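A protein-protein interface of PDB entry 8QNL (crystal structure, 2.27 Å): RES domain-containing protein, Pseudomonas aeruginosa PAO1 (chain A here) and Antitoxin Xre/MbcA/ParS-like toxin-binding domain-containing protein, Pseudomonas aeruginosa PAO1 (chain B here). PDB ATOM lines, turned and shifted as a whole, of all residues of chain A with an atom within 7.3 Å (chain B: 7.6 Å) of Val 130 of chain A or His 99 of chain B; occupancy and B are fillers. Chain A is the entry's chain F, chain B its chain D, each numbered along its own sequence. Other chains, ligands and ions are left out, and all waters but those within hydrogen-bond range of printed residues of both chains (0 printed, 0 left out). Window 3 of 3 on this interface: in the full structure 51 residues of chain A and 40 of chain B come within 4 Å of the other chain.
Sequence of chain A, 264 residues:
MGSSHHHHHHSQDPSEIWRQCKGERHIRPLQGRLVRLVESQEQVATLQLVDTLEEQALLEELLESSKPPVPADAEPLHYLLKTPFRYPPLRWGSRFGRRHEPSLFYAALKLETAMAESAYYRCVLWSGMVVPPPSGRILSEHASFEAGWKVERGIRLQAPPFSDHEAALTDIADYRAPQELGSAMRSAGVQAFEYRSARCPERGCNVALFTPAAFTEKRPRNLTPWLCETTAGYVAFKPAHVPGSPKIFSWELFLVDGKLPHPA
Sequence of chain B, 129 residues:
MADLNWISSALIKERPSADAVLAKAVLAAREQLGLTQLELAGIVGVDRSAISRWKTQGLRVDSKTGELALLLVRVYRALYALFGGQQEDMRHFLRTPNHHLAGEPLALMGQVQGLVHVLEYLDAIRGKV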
ATOM      1  N   TRP A  92       5.597   8.619  -4.209  1.00  0.00           N
ATOM      2  CA  TRP A  92       6.159   7.376  -4.719  1.00  0.00           C
ATOM      3  C   TRP A  92       5.862   6.201  -3.800  1.00  0.00           C
ATOM      4  O   TRP A  92       6.452   5.129  -3.967  1.00  0.00           O
ATOM      5  CB  TRP A  92       7.671   7.510  -4.939  1.00  0.00           C
ATOM      6  CG  TRP A  92       8.474   7.816  -3.707  1.00  0.00           C
ATOM      7  CD1 TRP A  92       8.853   6.938  -2.732  1.00  0.00           C
ATOM      8  CD2 TRP A  92       9.028   9.084  -3.340  1.00  0.00           C
ATOM      9  NE1 TRP A  92       9.596   7.585  -1.775  1.00  0.00           N
ATOM     10  CE2 TRP A  92       9.719   8.903  -2.126  1.00  0.00           C
ATOM     11  CE3 TRP A  92       9.000  10.358  -3.917  1.00  0.00           C
ATOM     12  CZ2 TRP A  92      10.377   9.947  -1.479  1.00  0.00           C
ATOM     13  CZ3 TRP A  92       9.653  11.393  -3.274  1.00  0.00           C
ATOM     14  CH2 TRP A  92      10.331  11.182  -2.067  1.00  0.00           C
ATOM     15  N   TRP A 126      16.463  16.914   3.337  1.00  0.00           N
ATOM     16  CA  TRP A 126      17.587  17.755   2.946  1.00  0.00           C
ATOM     17  C   TRP A 126      17.892  17.607   1.459  1.00  0.00           C
ATOM     18  O   TRP A 126      18.111  18.605   0.762  1.00  0.00           O
ATOM     19  CB  TRP A 126      18.811  17.404   3.796  1.00  0.00           C
ATOM     20  CG  TRP A 126      19.973  18.331   3.627  1.00  0.00           C
ATOM     21  CD1 TRP A 126      20.797  18.423   2.543  1.00  0.00           C
ATOM     22  CD2 TRP A 126      20.460  19.282   4.582  1.00  0.00           C
ATOM     23  NE1 TRP A 126      21.757  19.379   2.758  1.00  0.00           N
ATOM     24  CE2 TRP A 126      21.574  19.922   4.002  1.00  0.00           C
ATOM     25  CE3 TRP A 126      20.061  19.658   5.870  1.00  0.00           C
ATOM     26  CZ2 TRP A 126      22.293  20.916   4.662  1.00  0.00           C
ATOM     27  CZ3 TRP A 126      20.776  20.645   6.526  1.00  0.00           C
ATOM     28  CH2 TRP A 126      21.880  21.262   5.921  1.00  0.00           C
ATOM     29  N   SER A 127      17.887  16.373   0.950  1.00  0.00           N
ATOM     30  CA  SER A 127      18.289  16.127  -0.431  1.00  0.00           C
ATOM     31  C   SER A 127      17.258  16.612  -1.445  1.00  0.00           C
ATOM     32  O   SER A 127      17.604  16.793  -2.617  1.00  0.00           O
ATOM     33  CB  SER A 127      18.560  14.637  -0.641  1.00  0.00           C
ATOM     34  OG  SER A 127      17.367  13.879  -0.547  1.00  0.00           O
ATOM     35  N   GLY A 128      16.008  16.822  -1.027  1.00  0.00           N
ATOM     36  CA  GLY A 128      15.004  17.310  -1.956  1.00  0.00           C
ATOM     37  C   GLY A 128      15.308  18.702  -2.477  1.00  0.00           C
ATOM     38  O   GLY A 128      15.009  19.023  -3.629  1.00  0.00           O
ATOM     39  N   MET A 129      15.895  19.550  -1.638  1.00  0.00           N
ATOM     40  CA  MET A 129      16.246  20.889  -2.086  1.00  0.00           C
ATOM     41  C   MET A 129      17.497  20.825  -2.955  1.00  0.00           C
ATOM     42  O   MET A 129      18.497  20.209  -2.573  1.00  0.00           O
ATOM     43  CB  MET A 129      16.461  21.811  -0.882  1.00  0.00           C
ATOM     44  CG  MET A 129      15.201  22.047  -0.050  1.00  0.00           C
ATOM     45  SD  MET A 129      15.561  22.707   1.590  1.00  0.00           S
ATOM     46  CE  MET A 129      16.160  21.242   2.426  1.00  0.00           C
ATOM     47  N   VAL A 130      17.432  21.437  -4.141  1.00  0.00           N
ATOM     48  CA  VAL A 130      18.584  21.398  -5.037  1.00  0.00           C
ATOM     49  C   VAL A 130      19.754  22.169  -4.437  1.00  0.00           C
ATOM     50  O   VAL A 130      20.918  21.807  -4.648  1.00  0.00           O
ATOM     51  CB  VAL A 130      18.215  21.922  -6.442  1.00  0.00           C
ATOM     52  CG1 VAL A 130      17.061  21.112  -7.031  1.00  0.00           C
ATOM     53  CG2 VAL A 130      17.866  23.404  -6.403  1.00  0.00           C
ATOM     54  N   VAL A 131      19.475  23.216  -3.676  1.00  0.00           N
ATOM     55  CA  VAL A 131      20.483  23.969  -2.932  1.00  0.00           C
ATOM     56  C   VAL A 131      20.222  23.744  -1.448  1.00  0.00           C
ATOM     57  O   VAL A 131      19.087  23.933  -0.999  1.00  0.00           O
ATOM     58  CB  VAL A 131      20.441  25.473  -3.271  1.00  0.00           C
ATOM     59  CG1 VAL A 131      21.394  26.252  -2.375  1.00  0.00           C
ATOM     60  CG2 VAL A 131      20.779  25.699  -4.740  1.00  0.00           C
ATOM     61  N   PRO A 132      21.220  23.338  -0.664  1.00  0.00           N
ATOM     62  CA  PRO A 132      20.981  23.036   0.759  1.00  0.00           C
ATOM     63  C   PRO A 132      20.539  24.273   1.520  1.00  0.00           C
ATOM     64  O   PRO A 132      20.780  25.403   1.069  1.00  0.00           O
ATOM     65  CB  PRO A 132      22.349  22.536   1.250  1.00  0.00           C
ATOM     66  CG  PRO A 132      23.334  23.109   0.280  1.00  0.00           C
ATOM     67  CD  PRO A 132      22.625  23.112  -1.044  1.00  0.00           C
ATOM     68  N   LYS A 259      25.410   9.735  -3.887  1.00  0.00           N
ATOM     69  CA  LYS A 259      24.288  10.500  -3.365  1.00  0.00           C
ATOM     70  C   LYS A 259      23.174   9.563  -2.905  1.00  0.00           C
ATOM     71  O   LYS A 259      23.097   8.402  -3.315  1.00  0.00           O
ATOM     72  CB  LYS A 259      23.770  11.494  -4.421  1.00  0.00           C
ATOM     73  CG  LYS A 259      22.673  12.444  -3.946  1.00  0.00           C
ATOM     74  CD  LYS A 259      23.087  13.225  -2.706  1.00  0.00           C
ATOM     75  CE  LYS A 259      21.875  13.814  -1.997  1.00  0.00           C
ATOM     76  NZ  LYS A 259      20.974  14.543  -2.936  1.00  0.00           N
ATOM     77  N   HIS A 262      16.557   7.269  -3.870  1.00  0.00           N
ATOM     78  CA  HIS A 262      15.147   7.288  -3.520  1.00  0.00           C
ATOM     79  C   HIS A 262      14.372   6.743  -4.710  1.00  0.00           C
ATOM     80  O   HIS A 262      14.773   6.982  -5.858  1.00  0.00           O
ATOM     81  CB  HIS A 262      14.655   8.696  -3.157  1.00  0.00           C
ATOM     82  CG  HIS A 262      14.276   9.530  -4.342  1.00  0.00           C
ATOM     83  ND1 HIS A 262      12.966   9.717  -4.728  1.00  0.00           N
ATOM     84  CD2 HIS A 262      15.032  10.222  -5.226  1.00  0.00           C
ATOM     85  CE1 HIS A 262      12.931  10.490  -5.799  1.00  0.00           C
ATOM     86  NE2 HIS A 262      14.171  10.810  -6.121  1.00  0.00           N
ATOM     87  N   HIS B  92      13.684  29.208   2.716  1.00  0.00           N
ATOM     88  CA  HIS B  92      14.521  28.627   1.672  1.00  0.00           C
ATOM     89  C   HIS B  92      13.811  27.476   0.974  1.00  0.00           C
ATOM     90  O   HIS B  92      13.852  27.370  -0.256  1.00  0.00           O
ATOM     91  CB  HIS B  92      15.848  28.159   2.266  1.00  0.00           C
ATOM     92  CG  HIS B  92      16.727  27.445   1.288  1.00  0.00           C
ATOM     93  ND1 HIS B  92      17.567  28.107   0.419  1.00  0.00           N
ATOM     94  CD2 HIS B  92      16.895  26.123   1.041  1.00  0.00           C
ATOM     95  CE1 HIS B  92      18.217  27.225  -0.319  1.00  0.00           C
ATOM     96  NE2 HIS B  92      17.825  26.015   0.036  1.00  0.00           N
ATOM     97  N   THR B  96      13.121  27.479  -3.196  1.00  0.00           N
ATOM     98  CA  THR B  96      14.175  26.725  -3.863  1.00  0.00           C
ATOM     99  C   THR B  96      13.571  25.576  -4.650  1.00  0.00           C
ATOM    100  O   THR B  96      12.700  24.867  -4.126  1.00  0.00           O
ATOM    101  CB  THR B  96      15.187  26.179  -2.843  1.00  0.00           C
ATOM    102  OG1 THR B  96      15.811  27.269  -2.156  1.00  0.00           O
ATOM    103  CG2 THR B  96      16.258  25.341  -3.534  1.00  0.00           C
ATOM    104  N   PRO B  97      13.987  25.369  -5.901  1.00  0.00           N
ATOM    105  CA  PRO B  97      13.491  24.214  -6.661  1.00  0.00           C
ATOM    106  C   PRO B  97      13.763  22.912  -5.920  1.00  0.00           C
ATOM    107  O   PRO B  97      14.817  22.730  -5.308  1.00  0.00           O
ATOM    108  CB  PRO B  97      14.274  24.293  -7.976  1.00  0.00           C
ATOM    109  CG  PRO B  97      14.629  25.739  -8.111  1.00  0.00           C
ATOM    110  CD  PRO B  97      14.858  26.237  -6.711  1.00  0.00           C
ATOM    111  N   ASN B  98      12.790  22.008  -5.972  1.00  0.00           N
ATOM    112  CA  ASN B  98      12.821  20.774  -5.201  1.00  0.00           C
ATOM    113  C   ASN B  98      12.827  19.574  -6.137  1.00  0.00           C
ATOM    114  O   ASN B  98      12.079  19.537  -7.119  1.00  0.00           O
ATOM    115  CB  ASN B  98      11.619  20.695  -4.251  1.00  0.00           C
ATOM    116  CG  ASN B  98      11.756  19.586  -3.233  1.00  0.00           C
ATOM    117  OD1 ASN B  98      11.447  18.429  -3.511  1.00  0.00           O
ATOM    118  ND2 ASN B  98      12.220  19.935  -2.038  1.00  0.00           N
ATOM    119  N   HIS B  99      13.668  18.587  -5.818  1.00  0.00           N
ATOM    120  CA  HIS B  99      13.745  17.384  -6.642  1.00  0.00           C
ATOM    121  C   HIS B  99      12.492  16.532  -6.501  1.00  0.00           C
ATOM    122  O   HIS B  99      11.966  16.021  -7.497  1.00  0.00           O
ATOM    123  CB  HIS B  99      14.977  16.561  -6.268  1.00  0.00           C
ATOM    124  CG  HIS B  99      16.270  17.159  -6.724  1.00  0.00           C
ATOM    125  ND1 HIS B  99      16.575  17.341  -8.055  1.00  0.00           N
ATOM    126  CD2 HIS B  99      17.342  17.604  -6.028  1.00  0.00           C
ATOM    127  CE1 HIS B  99      17.777  17.878  -8.160  1.00  0.00           C
ATOM    128  NE2 HIS B  99      18.265  18.047  -6.944  1.00  0.00           N
ATOM    129  N   HIS B 100      12.013  16.358  -5.268  1.00  0.00           N
ATOM    130  CA  HIS B 100      10.883  15.473  -5.007  1.00  0.00           C
ATOM    131  C   HIS B 100       9.561  16.085  -5.446  1.00  0.00           C
ATOM    132  O   HIS B 100       8.637  15.353  -5.819  1.00  0.00           O
ATOM    133  CB  HIS B 100      10.842  15.119  -3.520  1.00  0.00           C
ATOM    134  CG  HIS B 100      12.122  14.539  -3.008  1.00  0.00           C
ATOM    135  ND1 HIS B 100      12.457  14.533  -1.672  1.00  0.00           N
ATOM    136  CD2 HIS B 100      13.156  13.949  -3.656  1.00  0.00           C
ATOM    137  CE1 HIS B 100      13.638  13.963  -1.518  1.00  0.00           C
ATOM    138  NE2 HIS B 100      14.084  13.598  -2.706  1.00  0.00           N
ATOM    139  N   LEU B 101       9.445  17.407  -5.397  1.00  0.00           N
ATOM    140  CA  LEU B 101       8.269  18.096  -5.892  1.00  0.00           C
ATOM    141  C   LEU B 101       8.474  18.485  -7.353  1.00  0.00           C
ATOM    142  O   LEU B 101       9.565  18.357  -7.915  1.00  0.00           O
ATOM    143  CB  LEU B 101       7.972  19.327  -5.036  1.00  0.00           C
ATOM    144  CG  LEU B 101       7.705  19.031  -3.557  1.00  0.00           C
ATOM    145  CD1 LEU B 101       7.755  20.294  -2.700  1.00  0.00           C
ATOM    146  CD2 LEU B 101       6.360  18.340  -3.411  1.00  0.00           C
ATOM    147  N   ALA B 102       7.399  18.968  -7.978  1.00  0.00           N
ATOM    148  CA  ALA B 102       7.460  19.297  -9.396  1.00  0.00           C
ATOM    149  C   ALA B 102       8.341  20.508  -9.691  1.00  0.00           C
ATOM    150  O   ALA B 102       8.676  20.736 -10.857  1.00  0.00           O
ATOM    151  CB  ALA B 102       6.047  19.532  -9.938  1.00  0.00           C
ATOM    152  N   GLY B 103       8.724  21.280  -8.675  1.00  0.00           N
ATOM    153  CA  GLY B 103       9.511  22.480  -8.878  1.00  0.00           C
ATOM    154  C   GLY B 103       9.645  23.296  -7.608  1.00  0.00           C
ATOM    155  O   GLY B 103       9.807  22.734  -6.520  1.00  0.00           O
ATOM    156  N   GLU B 104       9.584  24.616  -7.729  1.00  0.00           N
ATOM    157  CA  GLU B 104       9.631  25.485  -6.556  1.00  0.00           C
ATOM    158  C   GLU B 104       8.322  25.372  -5.781  1.00  0.00           C
ATOM    159  O   GLU B 104       7.254  25.618  -6.356  1.00  0.00           O
ATOM    160  CB  GLU B 104       9.873  26.932  -6.974  1.00  0.00           C
ATOM    161  CG  GLU B 104      10.185  27.864  -5.817  1.00  0.00           C
ATOM    162  CD  GLU B 104       9.891  29.317  -6.138  1.00  0.00           C
ATOM    163  OE1 GLU B 104       8.866  29.590  -6.801  1.00  0.00           O
ATOM    164  OE2 GLU B 104      10.685  30.190  -5.727  1.00  0.00           O
ATOM    165  N   TYR B 121       3.387  16.323   0.762  1.00  0.00           N
ATOM    166  CA  TYR B 121       4.793  15.962   0.915  1.00  0.00           C
ATOM    167  C   TYR B 121       5.299  16.294   2.314  1.00  0.00           C
ATOM    168  O   TYR B 121       6.001  15.486   2.934  1.00  0.00           O
ATOM    169  CB  TYR B 121       5.637  16.674  -0.145  1.00  0.00           C
ATOM    170  CG  TYR B 121       7.134  16.496   0.019  1.00  0.00           C
ATOM    171  CD1 TYR B 121       7.779  15.377  -0.492  1.00  0.00           C
ATOM    172  CD2 TYR B 121       7.904  17.452   0.675  1.00  0.00           C
ATOM    173  CE1 TYR B 121       9.148  15.206  -0.348  1.00  0.00           C
ATOM    174  CE2 TYR B 121       9.276  17.290   0.826  1.00  0.00           C
ATOM    175  CZ  TYR B 121       9.892  16.164   0.309  1.00  0.00           C
ATOM    176  OH  TYR B 121      11.252  15.983   0.448  1.00  0.00           O
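Among the printed residues, pairs that only touch across the chains: Trp 92 of chain A with His 100 of chain B, Ser 127 of chain A with His 99 of chain B, Ser 127 of chain A with His 100 of chain B, Gly 128 of chain A with His 100 of chain B, Met 129 of chain A with His 92 of chain B, Met 129 of chain A with Pro 97 of chain B, Met 129 of chain A with Asn 98 of chain B, Val 130 of chain A with Thr 96 of chain B, Val 130 of chain A with His 99 of chain B and Val 131 of chain A with Thr 96 of chain B.
NE2 of His 92 of chain B lies within hydrogen-bond range of O of Pro 132 of chain A.
The backbone NH (N) of His 99 of chain B lies within hydrogen-bond range of the backbone carbonyl oxygen (O) of Gly 128 of chain A (2.6 Å).
O of Gly 128 of chain A lies close to ND2 of Asn 98 of chain B (3.3 Å).
The backbone NH (N) of Val 130 of chain A lies within hydrogen-bond range of the backbone carbonyl oxygen (O) of Pro 97 of chain B, at 3.1 Å.
O of Val 131 of chain A lies within hydrogen-bond range of NE2 of His 92 of chain B, 2.6 Å away.
Of chain B, only Thr 96, Pro 97 and His 99 come within 4 Å of Val 130 of chain A.
Of the printed residues of chain B, Gly 128 of chain A touches Asn 98, His 99 and His 100.
Of the printed residues of chain A, Asn 98 of chain B touches Gly 128 and Met 129.
Of the printed residues of chain A, Pro 97 of chain B touches Met 129 (3.98 Å) and Val 130 (3.1 Å).
Of the printed residues of chain B, Val 131 of chain A touches His 92 (2.6 Å) and Thr 96 (3.9 Å).
The nearest residue of chain B that does not touch Val 130 of chain A is Asn 98 of chain B (4.5 Å).
Of the 11 printed residues of chain B, 6 touch a printed residue of chain A.
Printed residues of chain B that touch a printed residue of chain A: His 92, Thr 96, Pro 97, Asn 98, His 99 and His 100.
Hydrophobic or aromatic side chains of chain B within 4 Å of the printed part of chain A: His 92, His 99 and His 100.
Of the 10 printed residues of chain A, 7 touch a printed residue of chain B.
Printed residues of chain A that touch a printed residue of chain B: Trp 92, Ser 127, Gly 128, Met 129, Val 130, Val 131 and Pro 132.
Hydrophobic or aromatic side chains of chain A that line the printed part of chain B: Trp 92, Met 129, Val 130 and Val 131.
Among the printed residues, 15 pairs touch across the chains.
Among the printed residues, no Asp or Glu carboxylate lies within 4 Å of a Lys or Arg side-chain nitrogen of the other chain.
OD1 of Asn 98 of chain B is in hydrogen-bond range of N of Leu 101 of chain B (2.9 Å).
The side-chain amide oxygen of Asn 98 of chain B is in hydrogen-bond range of the backbone NH of His 100 of chain B, at 2.8 Å.
N of Asn 98 of chain B lies within hydrogen-bond range of O of Gly 103 of chain B, at 3.1 Å.
A ring nitrogen (ND1) of His 100 of chain B is in hydrogen-bond range of the side-chain hydroxyl of Tyr 121 of chain B (2.8 Å).
OG1 of Thr 96 of chain B lies within hydrogen-bond range of O of His 92 of chain B.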
